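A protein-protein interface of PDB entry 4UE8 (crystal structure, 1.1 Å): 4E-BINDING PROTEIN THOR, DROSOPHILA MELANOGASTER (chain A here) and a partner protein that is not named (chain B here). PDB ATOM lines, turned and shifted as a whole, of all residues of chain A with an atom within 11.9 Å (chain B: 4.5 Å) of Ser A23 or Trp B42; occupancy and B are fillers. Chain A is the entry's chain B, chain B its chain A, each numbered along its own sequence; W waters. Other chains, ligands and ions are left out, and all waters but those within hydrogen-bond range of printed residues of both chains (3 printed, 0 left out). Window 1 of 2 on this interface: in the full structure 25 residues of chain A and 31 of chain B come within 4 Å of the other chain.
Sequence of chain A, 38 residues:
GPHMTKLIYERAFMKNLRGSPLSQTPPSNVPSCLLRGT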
ATOM      1  N   TYR A   9       9.557  11.881  11.684  1.00  0.00           N
ATOM      2  CA  TYR A   9       9.534  13.336  11.703  1.00  0.00           C
ATOM      3  C   TYR A   9       8.574  13.838  12.750  1.00  0.00           C
ATOM      4  O   TYR A   9       7.457  13.325  12.901  1.00  0.00           O
ATOM      5  CB  TYR A   9       9.072  13.918  10.377  1.00  0.00           C
ATOM      6  CG  TYR A   9       9.945  13.604   9.187  1.00  0.00           C
ATOM      7  CD1 TYR A   9      11.199  14.186   9.032  1.00  0.00           C
ATOM      8  CD2 TYR A   9       9.514  12.747   8.202  1.00  0.00           C
ATOM      9  CE1 TYR A   9      11.982  13.908   7.933  1.00  0.00           C
ATOM     10  CE2 TYR A   9      10.277  12.481   7.094  1.00  0.00           C
ATOM     11  CZ  TYR A   9      11.514  13.069   6.958  1.00  0.00           C
ATOM     12  OH  TYR A   9      12.290  12.821   5.854  1.00  0.00           O
ATOM     13  N   GLU A  10       8.998  14.885  13.435  1.00  0.00           N
ATOM     14  CA  GLU A  10       8.114  15.637  14.304  1.00  0.00           C
ATOM     15  C   GLU A  10       7.197  16.530  13.493  1.00  0.00           C
ATOM     16  O   GLU A  10       7.532  16.979  12.388  1.00  0.00           O
ATOM     17  CB  GLU A  10       8.931  16.498  15.246  1.00  0.00           C
ATOM     18  CG  GLU A  10       9.829  15.678  16.147  1.00  0.00           C
ATOM     19  CD  GLU A  10      10.606  16.517  17.136  1.00  0.00           C
ATOM     20  OE1 GLU A  10      10.992  17.653  16.789  1.00  0.00           O
ATOM     21  OE2 GLU A  10      10.834  16.033  18.265  1.00  0.00           O
ATOM     22  N   ARG A  11       6.047  16.820  14.077  1.00  0.00           N
ATOM     23  CA  ARG A  11       5.074  17.666  13.423  1.00  0.00           C
ATOM     24  C   ARG A  11       5.651  19.026  13.067  1.00  0.00           C
ATOM     25  O   ARG A  11       5.421  19.517  11.972  1.00  0.00           O
ATOM     26  CB  ARG A  11       3.854  17.827  14.321  1.00  0.00           C
ATOM     27  CG  ARG A  11       2.960  16.609  14.298  1.00  0.00           C
ATOM     28  CD  ARG A  11       1.703  16.835  15.100  1.00  0.00           C
ATOM     29  NE  ARG A  11       1.984  16.916  16.527  1.00  0.00           N
ATOM     30  CZ  ARG A  11       1.071  17.182  17.451  1.00  0.00           C
ATOM     31  NH1 ARG A  11      -0.191  17.388  17.100  1.00  0.00           N
ATOM     32  NH2 ARG A  11       1.418  17.241  18.728  1.00  0.00           N
ATOM     33  N   ALA A  12       6.385  19.637  13.995  1.00  0.00           N
ATOM     34  CA  ALA A  12       6.889  20.993  13.750  1.00  0.00           C
ATOM     35  C   ALA A  12       7.858  21.008  12.570  1.00  0.00           C
ATOM     36  O   ALA A  12       7.846  21.929  11.749  1.00  0.00           O
ATOM     37  CB  ALA A  12       7.559  21.559  14.994  1.00  0.00           C
ATOM     38  N   PHE A  13       8.700  19.990  12.489  1.00  0.00           N
ATOM     39  CA  PHE A  13       9.657  19.892  11.394  1.00  0.00           C
ATOM     40  C   PHE A  13       8.916  19.858  10.057  1.00  0.00           C
ATOM     41  O   PHE A  13       9.292  20.556   9.112  1.00  0.00           O
ATOM     42  CB  PHE A  13      10.528  18.647  11.545  1.00  0.00           C
ATOM     43  CG  PHE A  13      11.532  18.488  10.443  1.00  0.00           C
ATOM     44  CD1 PHE A  13      12.785  19.071  10.540  1.00  0.00           C
ATOM     45  CD2 PHE A  13      11.218  17.778   9.298  1.00  0.00           C
ATOM     46  CE1 PHE A  13      13.707  18.935   9.518  1.00  0.00           C
ATOM     47  CE2 PHE A  13      12.134  17.643   8.267  1.00  0.00           C
ATOM     48  CZ  PHE A  13      13.376  18.232   8.376  1.00  0.00           C
ATOM     49  N   MET A  14       7.873  19.043   9.976  1.00  0.00           N
ATOM     50  CA  MET A  14       7.105  18.949   8.745  1.00  0.00           C
ATOM     51  C   MET A  14       6.342  20.232   8.450  1.00  0.00           C
ATOM     52  O   MET A  14       6.313  20.666   7.299  1.00  0.00           O
ATOM     53  CB  MET A  14       6.180  17.740   8.776  1.00  0.00           C
ATOM     54  CG  MET A  14       6.957  16.438   8.744  1.00  0.00           C
ATOM     55  SD  MET A  14       5.905  14.973   8.604  1.00  0.00           S
ATOM     56  CE  MET A  14       5.257  14.913  10.264  1.00  0.00           C
ATOM     57  N   LYS A  15       5.744  20.859   9.466  1.00  0.00           N
ATOM     58  CA  LYS A  15       5.019  22.103   9.245  1.00  0.00           C
ATOM     59  C   LYS A  15       5.956  23.198   8.734  1.00  0.00           C
ATOM     60  O   LYS A  15       5.529  24.041   7.946  1.00  0.00           O
ATOM     61  CB  LYS A  15       4.246  22.531  10.492  1.00  0.00           C
ATOM     62  CG  LYS A  15       3.024  21.667  10.719  1.00  0.00           C
ATOM     63  CD  LYS A  15       2.206  22.138  11.891  1.00  0.00           C
ATOM     64  CE  LYS A  15       0.976  21.276  12.094  1.00  0.00           C
ATOM     65  NZ  LYS A  15       0.125  21.763  13.201  1.00  0.00           N
ATOM     66  N   ASN A  16       7.219  23.181   9.148  1.00  0.00           N
ATOM     67  CA  ASN A  16       8.180  24.174   8.689  1.00  0.00           C
ATOM     68  C   ASN A  16       8.526  24.024   7.211  1.00  0.00           C
ATOM     69  O   ASN A  16       9.083  24.940   6.618  1.00  0.00           O
ATOM     70  CB  ASN A  16       9.451  24.142   9.546  1.00  0.00           C
ATOM     71  CG  ASN A  16       9.226  24.685  10.952  1.00  0.00           C
ATOM     72  OD1 ASN A  16       8.249  25.384  11.212  1.00  0.00           O
ATOM     73  ND2 ASN A  16      10.134  24.358  11.864  1.00  0.00           N
ATOM     74  N   LEU A  17       8.171  22.890   6.617  1.00  0.00           N
ATOM     75  CA  LEU A  17       8.352  22.655   5.187  1.00  0.00           C
ATOM     76  C   LEU A  17       7.114  22.993   4.357  1.00  0.00           C
ATOM     77  O   LEU A  17       7.158  22.908   3.138  1.00  0.00           O
ATOM     78  CB  LEU A  17       8.757  21.205   4.918  1.00  0.00           C
ATOM     79  CG  LEU A  17      10.142  20.817   5.423  1.00  0.00           C
ATOM     80  CD1 LEU A  17      10.320  19.304   5.352  1.00  0.00           C
ATOM     81  CD2 LEU A  17      11.242  21.526   4.644  1.00  0.00           C
ATOM     82  N   ARG A  18       6.015  23.393   4.999  1.00  0.00           N
ATOM     83  CA  ARG A  18       4.767  23.614   4.274  1.00  0.00           C
ATOM     84  C   ARG A  18       4.845  24.726   3.234  1.00  0.00           C
ATOM     85  O   ARG A  18       4.169  24.660   2.206  1.00  0.00           O
ATOM     86  CB  ARG A  18       3.638  23.901   5.254  1.00  0.00           C
ATOM     87  CG  ARG A  18       2.299  23.982   4.585  1.00  0.00           C
ATOM     88  CD  ARG A  18       1.177  24.064   5.576  1.00  0.00           C
ATOM     89  NE  ARG A  18      -0.091  23.961   4.871  1.00  0.00           N
ATOM     90  CZ  ARG A  18      -1.290  23.945   5.439  1.00  0.00           C
ATOM     91  NH1 ARG A  18      -1.427  24.043   6.756  1.00  0.00           N
ATOM     92  NH2 ARG A  18      -2.356  23.824   4.667  1.00  0.00           N
ATOM     93  N   GLY A  19       5.671  25.732   3.501  1.00  0.00           N
ATOM     94  CA  GLY A  19       5.857  26.842   2.585  1.00  0.00           C
ATOM     95  C   GLY A  19       7.005  26.692   1.604  1.00  0.00           C
ATOM     96  O   GLY A  19       7.247  27.603   0.821  1.00  0.00           O
ATOM     97  N   SER A  20       7.694  25.552   1.629  1.00  0.00           N
ATOM     98  CA  SER A  20       8.830  25.320   0.741  1.00  0.00           C
ATOM     99  C   SER A  20       8.405  25.404  -0.710  1.00  0.00           C
ATOM    100  O   SER A  20       7.282  25.055  -1.045  1.00  0.00           O
ATOM    101  CB  SER A  20       9.393  23.915   0.981  1.00  0.00           C
ATOM    102  OG  SER A  20      10.220  23.478  -0.089  1.00  0.00           O
ATOM    103  N   PRO A  21       9.325  25.780  -1.600  1.00  0.00           N
ATOM    104  CA  PRO A  21       8.920  25.789  -3.010  1.00  0.00           C
ATOM    105  C   PRO A  21       8.488  24.416  -3.525  1.00  0.00           C
ATOM    106  O   PRO A  21       7.594  24.314  -4.356  1.00  0.00           O
ATOM    107  CB  PRO A  21      10.162  26.305  -3.745  1.00  0.00           C
ATOM    108  CG  PRO A  21      11.277  26.213  -2.786  1.00  0.00           C
ATOM    109  CD  PRO A  21      10.709  26.244  -1.406  1.00  0.00           C
ATOM    110  N   LEU A  22       9.077  23.364  -2.971  1.00  0.00           N
ATOM    111  CA  LEU A  22       8.744  21.999  -3.369  1.00  0.00           C
ATOM    112  C   LEU A  22       7.398  21.522  -2.819  1.00  0.00           C
ATOM    113  O   LEU A  22       6.922  20.450  -3.191  1.00  0.00           O
ATOM    114  CB  LEU A  22       9.856  21.047  -2.926  1.00  0.00           C
ATOM    115  CG  LEU A  22      11.285  21.435  -3.332  1.00  0.00           C
ATOM    116  CD1 LEU A  22      12.326  20.429  -2.837  1.00  0.00           C
ATOM    117  CD2 LEU A  22      11.379  21.595  -4.844  1.00  0.00           C
ATOM    118  N   SER A  23       6.795  22.310  -1.934  1.00  0.00           N
ATOM    119  CA  SER A  23       5.506  21.979  -1.330  1.00  0.00           C
ATOM    120  C   SER A  23       4.334  22.677  -2.020  1.00  0.00           C
ATOM    121  O   SER A  23       3.200  22.632  -1.528  1.00  0.00           O
ATOM    122  CB  SER A  23       5.523  22.376   0.134  1.00  0.00           C
ATOM    123  OG  SER A  23       6.366  21.514   0.861  1.00  0.00           O
ATOM    124  N   GLN A  24       4.616  23.336  -3.144  1.00  0.00           N
ATOM    125  CA  GLN A  24       3.606  24.120  -3.866  1.00  0.00           C
ATOM    126  C   GLN A  24       3.264  23.561  -5.242  1.00  0.00           C
ATOM    127  O   GLN A  24       2.684  24.268  -6.058  1.00  0.00           O
ATOM    128  CB  GLN A  24       4.033  25.588  -4.044  1.00  0.00           C
ATOM    129  CG  GLN A  24       4.661  26.234  -2.828  1.00  0.00           C
ATOM    130  CD  GLN A  24       3.835  26.081  -1.584  1.00  0.00           C
ATOM    131  OE1 GLN A  24       2.605  26.195  -1.610  1.00  0.00           O
ATOM    132  NE2 GLN A  24       4.505  25.794  -0.477  1.00  0.00           N
ATOM    133  N   THR A  25       3.599  22.306  -5.513  1.00  0.00           N
ATOM    134  CA  THR A  25       3.362  21.744  -6.839  1.00  0.00           C
ATOM    135  C   THR A  25       1.915  21.299  -6.989  1.00  0.00           C
ATOM    136  O   THR A  25       1.457  20.439  -6.241  1.00  0.00           O
ATOM    137  CB  THR A  25       4.252  20.532  -7.079  1.00  0.00           C
ATOM    138  OG1 THR A  25       5.615  20.907  -6.864  1.00  0.00           O
ATOM    139  CG2 THR A  25       4.083  20.007  -8.496  1.00  0.00           C
ATOM    140  N   PRO A  26       1.181  21.882  -7.950  1.00  0.00           N
ATOM    141  CA  PRO A  26      -0.190  21.390  -8.140  1.00  0.00           C
ATOM    142  C   PRO A  26      -0.208  19.878  -8.388  1.00  0.00           C
ATOM    143  O   PRO A  26       0.531  19.402  -9.248  1.00  0.00           O
ATOM    144  CB  PRO A  26      -0.666  22.150  -9.381  1.00  0.00           C
ATOM    145  CG  PRO A  26       0.160  23.390  -9.406  1.00  0.00           C
ATOM    146  CD  PRO A  26       1.504  22.983  -8.877  1.00  0.00           C
ATOM    147  N   PRO A  27      -1.010  19.122  -7.621  1.00  0.00           N
ATOM    148  CA  PRO A  27      -1.032  17.669  -7.825  1.00  0.00           C
ATOM    149  C   PRO A  27      -1.733  17.314  -9.134  1.00  0.00           C
ATOM    150  O   PRO A  27      -2.774  17.884  -9.446  1.00  0.00           O
ATOM    151  CB  PRO A  27      -1.815  17.159  -6.607  1.00  0.00           C
ATOM    152  CG  PRO A  27      -2.697  18.295  -6.234  1.00  0.00           C
ATOM    153  CD  PRO A  27      -1.919  19.541  -6.539  1.00  0.00           C
ATOM    154  N   SER A  28      -1.167  16.375  -9.884  1.00  0.00           N
ATOM    155  CA  SER A  28      -1.580  16.149 -11.268  1.00  0.00           C
ATOM    156  C   SER A  28      -2.929  15.436 -11.426  1.00  0.00           C
ATOM    157  O   SER A  28      -3.763  15.850 -12.231  1.00  0.00           O
ATOM    158  CB  SER A  28      -0.494  15.362 -12.005  1.00  0.00           C
ATOM    159  OG  SER A  28      -0.842  15.161 -13.362  1.00  0.00           O
ATOM    160  N   VAL A  30      -5.759  14.996  -9.696  1.00  0.00           N
ATOM    161  CA  VAL A  30      -6.822  15.314  -8.737  1.00  0.00           C
ATOM    162  C   VAL A  30      -8.097  15.825  -9.423  1.00  0.00           C
ATOM    163  O   VAL A  30      -8.047  16.802 -10.171  1.00  0.00           O
ATOM    164  CB  VAL A  30      -6.340  16.348  -7.707  1.00  0.00           C
ATOM    165  CG1 VAL A  30      -7.437  16.660  -6.693  1.00  0.00           C
ATOM    166  CG2 VAL A  30      -5.104  15.823  -6.997  1.00  0.00           C
ATOM    167  N   LEU A  34     -12.265  18.298  -6.035  1.00  0.00           N
ATOM    168  CA  LEU A  34     -11.495  18.313  -4.792  1.00  0.00           C
ATOM    169  C   LEU A  34     -10.540  19.479  -4.686  1.00  0.00           C
ATOM    170  O   LEU A  34      -9.875  19.613  -3.674  1.00  0.00           O
ATOM    171  CB  LEU A  34     -10.703  17.017  -4.628  1.00  0.00           C
ATOM    172  CG  LEU A  34     -11.535  15.760  -4.413  1.00  0.00           C
ATOM    173  CD1 LEU A  34     -10.630  14.562  -4.225  1.00  0.00           C
ATOM    174  CD2 LEU A  34     -12.441  15.909  -3.203  1.00  0.00           C
ATOM    175  N   LEU A  35     -10.448  20.324  -5.700  1.00  0.00           N
ATOM    176  CA  LEU A  35      -9.491  21.418  -5.622  1.00  0.00           C
ATOM    177  C   LEU A  35     -10.011  22.562  -4.756  1.00  0.00           C
ATOM    178  O   LEU A  35     -11.191  22.892  -4.773  1.00  0.00           O
ATOM    179  CB  LEU A  35      -9.096  21.894  -7.024  1.00  0.00           C
ATOM    180  CG  LEU A  35      -8.332  20.843  -7.846  1.00  0.00           C
ATOM    181  CD1 LEU A  35      -8.119  21.320  -9.275  1.00  0.00           C
ATOM    182  CD2 LEU A  35      -6.993  20.492  -7.206  1.00  0.00           C
ATOM    183  N   ARG A  36      -9.110  23.158  -3.984  1.00  0.00           N
ATOM    184  CA  ARG A  36      -9.454  24.316  -3.165  1.00  0.00           C
ATOM    185  C   ARG A  36     -10.077  25.431  -3.973  1.00  0.00           C
ATOM    186  O   ARG A  36      -9.589  25.769  -5.048  1.00  0.00           O
ATOM    187  CB  ARG A  36      -8.215  24.891  -2.495  1.00  0.00           C
ATOM    188  CG  ARG A  36      -8.027  24.405  -1.113  1.00  0.00           C
ATOM    189  CD  ARG A  36      -6.787  24.979  -0.482  1.00  0.00           C
ATOM    190  NE  ARG A  36      -6.334  24.099   0.588  1.00  0.00           N
ATOM    191  CZ  ARG A  36      -6.479  24.328   1.889  1.00  0.00           C
ATOM    192  NH1 ARG A  36      -7.037  25.443   2.334  1.00  0.00           N
ATOM    193  NH2 ARG A  36      -6.029  23.434   2.758  1.00  0.00           N
ATOM    194  N   VAL B  38       7.578  14.477   2.345  1.00  0.00           N
ATOM    195  CA  VAL B  38       6.866  15.505   3.087  1.00  0.00           C
ATOM    196  C   VAL B  38       6.340  16.578   2.129  1.00  0.00           C
ATOM    197  O   VAL B  38       5.201  17.038   2.255  1.00  0.00           O
ATOM    198  CB  VAL B  38       7.778  16.150   4.154  1.00  0.00           C
ATOM    199  CG1 VAL B  38       7.045  17.272   4.877  1.00  0.00           C
ATOM    200  CG2 VAL B  38       8.298  15.107   5.145  1.00  0.00           C
ATOM    201  N   GLU B  39       7.178  17.004   1.194  1.00  0.00           N
ATOM    202  CA  GLU B  39       6.804  18.070   0.278  1.00  0.00           C
ATOM    203  C   GLU B  39       5.715  17.658  -0.695  1.00  0.00           C
ATOM    204  O   GLU B  39       4.863  18.474  -1.044  1.00  0.00           O
ATOM    205  CB  GLU B  39       8.026  18.588  -0.486  1.00  0.00           C
ATOM    206  CG  GLU B  39       9.045  19.276   0.416  1.00  0.00           C
ATOM    207  CD  GLU B  39      10.067  18.355   1.064  1.00  0.00           C
ATOM    208  OE1 GLU B  39       9.897  17.114   1.111  1.00  0.00           O
ATOM    209  OE2 GLU B  39      11.078  18.900   1.544  1.00  0.00           O
ATOM    210  N   ASP B  40       5.713  16.405  -1.127  1.00  0.00           N
ATOM    211  CA  ASP B  40       4.620  15.923  -1.963  1.00  0.00           C
ATOM    212  C   ASP B  40       3.321  15.812  -1.165  1.00  0.00           C
ATOM    213  O   ASP B  40       2.247  16.060  -1.709  1.00  0.00           O
ATOM    214  CB  ASP B  40       4.986  14.617  -2.667  1.00  0.00           C
ATOM    215  CG  ASP B  40       6.124  14.803  -3.645  1.00  0.00           C
ATOM    216  OD1 ASP B  40       6.155  15.828  -4.356  1.00  0.00           O
ATOM    217  OD2 ASP B  40       7.019  13.931  -3.673  1.00  0.00           O
ATOM    218  N   PHE B  41       3.404  15.469   0.117  1.00  0.00           N
ATOM    219  CA  PHE B  41       2.237  15.544   0.977  1.00  0.00           C
ATOM    220  C   PHE B  41       1.701  16.973   0.991  1.00  0.00           C
ATOM    221  O   PHE B  41       0.507  17.195   0.792  1.00  0.00           O
ATOM    222  CB  PHE B  41       2.558  15.103   2.411  1.00  0.00           C
ATOM    223  CG  PHE B  41       1.476  15.496   3.367  1.00  0.00           C
ATOM    224  CD1 PHE B  41       0.263  14.837   3.356  1.00  0.00           C
ATOM    225  CD2 PHE B  41       1.644  16.562   4.225  1.00  0.00           C
ATOM    226  CE1 PHE B  41      -0.764  15.234   4.195  1.00  0.00           C
ATOM    227  CE2 PHE B  41       0.617  16.968   5.067  1.00  0.00           C
ATOM    228  CZ  PHE B  41      -0.587  16.294   5.062  1.00  0.00           C
ATOM    229  N   TRP B  42       2.560  17.951   1.262  1.00  0.00           N
ATOM    230  CA  TRP B  42       2.077  19.330   1.335  1.00  0.00           C
ATOM    231  C   TRP B  42       1.552  19.816  -0.001  1.00  0.00           C
ATOM    232  O   TRP B  42       0.566  20.537  -0.039  1.00  0.00           O
ATOM    233  CB  TRP B  42       3.150  20.293   1.829  1.00  0.00           C
ATOM    234  CG  TRP B  42       3.472  20.179   3.281  1.00  0.00           C
ATOM    235  CD1 TRP B  42       4.691  19.928   3.823  1.00  0.00           C
ATOM    236  CD2 TRP B  42       2.558  20.317   4.385  1.00  0.00           C
ATOM    237  NE1 TRP B  42       4.606  19.893   5.181  1.00  0.00           N
ATOM    238  CE2 TRP B  42       3.314  20.139   5.561  1.00  0.00           C
ATOM    239  CE3 TRP B  42       1.195  20.604   4.496  1.00  0.00           C
ATOM    240  CZ2 TRP B  42       2.752  20.213   6.829  1.00  0.00           C
ATOM    241  CZ3 TRP B  42       0.636  20.680   5.765  1.00  0.00           C
ATOM    242  CH2 TRP B  42       1.413  20.487   6.910  1.00  0.00           C
ATOM    243  N   SER B  43       2.180  19.417  -1.098  1.00  0.00           N
ATOM    244  CA  SER B  43       1.701  19.827  -2.415  1.00  0.00           C
ATOM    245  C   SER B  43       0.262  19.368  -2.617  1.00  0.00           C
ATOM    246  O   SER B  43      -0.578  20.096  -3.135  1.00  0.00           O
ATOM    247  CB  SER B  43       2.615  19.241  -3.484  1.00  0.00           C
ATOM    248  OG  SER B  43       3.846  19.962  -3.571  1.00  0.00           O
ATOM    249  N   LEU B  44      -0.028  18.152  -2.186  1.00  0.00           N
ATOM    250  CA  LEU B  44      -1.386  17.637  -2.247  1.00  0.00           C
ATOM    251  C   LEU B  44      -2.305  18.363  -1.267  1.00  0.00           C
ATOM    252  O   LEU B  44      -3.357  18.885  -1.662  1.00  0.00           O
ATOM    253  CB  LEU B  44      -1.365  16.137  -1.949  1.00  0.00           C
ATOM    254  CG  LEU B  44      -2.728  15.448  -1.866  1.00  0.00           C
ATOM    255  CD1 LEU B  44      -3.455  15.520  -3.194  1.00  0.00           C
ATOM    256  CD2 LEU B  44      -2.530  14.014  -1.427  1.00  0.00           C
ATOM    257  N   TYR B  45      -1.931  18.388   0.005  1.00  0.00           N
ATOM    258  CA  TYR B  45      -2.784  18.961   1.035  1.00  0.00           C
ATOM    259  C   TYR B  45      -3.093  20.434   0.773  1.00  0.00           C
ATOM    260  O   TYR B  45      -4.219  20.886   0.979  1.00  0.00           O
ATOM    261  CB  TYR B  45      -2.136  18.770   2.418  1.00  0.00           C
ATOM    262  CG  TYR B  45      -3.109  19.058   3.526  1.00  0.00           C
ATOM    263  CD1 TYR B  45      -4.005  18.084   3.949  1.00  0.00           C
ATOM    264  CD2 TYR B  45      -3.177  20.301   4.110  1.00  0.00           C
ATOM    265  CE1 TYR B  45      -4.951  18.342   4.911  1.00  0.00           C
ATOM    266  CE2 TYR B  45      -4.131  20.573   5.100  1.00  0.00           C
ATOM    267  CZ  TYR B  45      -5.015  19.580   5.486  1.00  0.00           C
ATOM    268  OH  TYR B  45      -5.975  19.793   6.455  1.00  0.00           O
ATOM    269  N   ASN B  46      -2.088  21.169   0.305  1.00  0.00           N
ATOM    270  CA  ASN B  46      -2.230  22.596   0.033  1.00  0.00           C
ATOM    271  C   ASN B  46      -3.169  22.881  -1.129  1.00  0.00           C
ATOM    272  O   ASN B  46      -3.713  23.978  -1.224  1.00  0.00           O
ATOM    273  CB  ASN B  46      -0.867  23.239  -0.258  1.00  0.00           C
ATOM    274  CG  ASN B  46      -0.023  23.446   0.989  1.00  0.00           C
ATOM    275  OD1 ASN B  46      -0.532  23.464   2.110  1.00  0.00           O
ATOM    276  ND2 ASN B  46       1.279  23.636   0.790  1.00  0.00           N
ATOM    277  N   LEU B  99      -5.349  17.448  10.077  1.00  0.00           N
ATOM    278  CA  LEU B  99      -3.983  17.622   9.626  1.00  0.00           C
ATOM    279  C   LEU B  99      -3.019  17.042  10.646  1.00  0.00           C
ATOM    280  O   LEU B  99      -2.061  16.349  10.283  1.00  0.00           O
ATOM    281  CB  LEU B  99      -3.689  19.102   9.379  1.00  0.00           C
ATOM    282  CG  LEU B  99      -2.247  19.415   8.983  1.00  0.00           C
ATOM    283  CD1 LEU B  99      -1.792  18.610   7.775  1.00  0.00           C
ATOM    284  CD2 LEU B  99      -2.121  20.895   8.698  1.00  0.00           C
ATOM    285  N   LEU B 103      -0.220  14.117  10.029  1.00  0.00           N
ATOM    286  CA  LEU B 103       1.186  14.294  10.339  1.00  0.00           C
ATOM    287  C   LEU B 103       1.687  13.239  11.328  1.00  0.00           C
ATOM    288  O   LEU B 103       2.826  12.780  11.211  1.00  0.00           O
ATOM    289  CB  LEU B 103       1.442  15.702  10.848  1.00  0.00           C
ATOM    290  CG  LEU B 103       1.221  16.802   9.807  1.00  0.00           C
ATOM    291  CD1 LEU B 103       1.438  18.161  10.428  1.00  0.00           C
ATOM    292  CD2 LEU B 103       2.112  16.627   8.571  1.00  0.00           C
HETATM  293  O   HOH W   1      -6.507  20.539   2.506  1.00  0.00           O
HETATM  294  O   HOH W   2      11.854  21.485   0.838  1.00  0.00           O
HETATM  295  O   HOH W   3       4.637  13.462  13.371  1.00  0.00           O
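The indole nitrogen (NE1) of Trp B42 lies within hydrogen-bond range of the backbone carbonyl oxygen (O) of Met A14, 2.8 Å away.
OG of Ser B43 lies within hydrogen-bond range of O of Leu A22 (3.1 Å).
The backbone NH of Ser B43 sits close to the backbone carbonyl oxygen of Ser A23, 3.4 Å away.
The side-chain hydroxyl (OG) of Ser B43 lies within hydrogen-bond range of the backbone NH (N) of Gln A24.
OG of Ser B43 is in hydrogen-bond range of N of Thr A25.
The side-chain amide oxygen (OD1) of Asn B46 is in hydrogen-bond range of the guanidinium group (NE) of Arg A18, at 2.8 Å.
The backbone carbonyl oxygen (O) of Ser A23 lies within hydrogen-bond range of the side-chain amide nitrogen (ND2) of Asn B46 (3.2 Å).
The backbone carbonyl oxygen (O) of Asn B46 sits at hydrogen-bond distance from the guanidinium group (NE) of Arg A36 (3.2 Å).
O of Glu B39 is in hydrogen-bond range of OG of Ser B43 (3.1 Å).
ND2 of Asn B46 sits close to O of Trp B42 (3.3 Å).
OG of Ser A23 lies within hydrogen-bond range of O of Leu A17.
The side-chain amide nitrogen (NE2) of Gln A24 is in hydrogen-bond range of the backbone carbonyl oxygen (O) of Arg A18, at 2.9 Å.
OG of Ser A20 sits at hydrogen-bond distance from N of Leu A22 (3.1 Å).
O of Ser A20 is in hydrogen-bond range of NE2 of Gln A24, at 2.9 Å.
Among the printed residues, merely in contact across the chains: Tyr A9 with Val B38, Arg A11 with Leu B103, Met A14 with Val B38, Met A14 with Leu B103, Lys A15 with Trp B42, Lys A15 with Leu B103, Leu A17 with Val B38, Leu A17 with Glu B39, Leu A17 with Trp B42, Arg A18 with Trp B42, Arg A18 with Tyr B45, Arg A18 with Leu B99, Leu A22 with Glu B39, Ser A23 with Glu B39, Ser A23 with Trp B42, Gln A24 with Asn B46, Pro A27 with Ser B43 and Arg A36 with Tyr B45.
Printed residues of chain B within 4 Å of Lys A15: Trp B42 and Leu B103.
Of the printed residues of chain B, Arg A18 touches Trp B42, Tyr B45, Asn B46 and Leu B99.
Gly A19 touches none of the printed residues of chain B.
Of chain B, only Glu B39, Trp B42, Ser B43 and Asn B46 come within 4 Å of Ser A23.
Of the printed residues of chain B, Thr A25 touches Ser B43.
Val A30 touches none of the printed residues of chain B.
Of chain A, only Tyr A9 (3.8 Å), Met A14 (3.96 Å) and Leu A17 (3.9 Å) come within 4 Å of Val B38.
No residue of chain A comes within 4 Å of Phe B41.
Tyr B45 touches two residues of chain A.
Of the printed residues of chain A, Leu B99 touches Arg A18 (3.8 Å).
The nearest printed residue of chain B that does not touch Ser A23 is Val B38 (4.8 Å).
Printed residues of chain B that touch a printed residue of chain A: Val B38, Glu B39, Trp B42, Ser B43, Tyr B45, Asn B46, Leu B99 and Leu B103.
Hydrophobic or aromatic side chains of chain A that line the printed part of chain B: Tyr A9, Met A14, Leu A17, Leu A22 and Pro A27.
Among the printed residues, 26 pairs touch across the chains.
Among the printed residues, no Asp or Glu carboxylate lies within 4 Å of a Lys or Arg side-chain nitrogen of the other chain.
Water W2 bridges the side-chain hydroxyl of Ser A20 (2.7 Å) and the side-chain carboxylate of Glu B39 (2.8 Å).
Water W1 bridges O of Tyr B45 (2.8 Å) and NH2 of Arg A36 (2.9 Å).
Water W3 lies within hydrogen-bond range of the backbone carbonyl oxygen of Tyr A9 and the backbone carbonyl oxygen of Leu B103.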
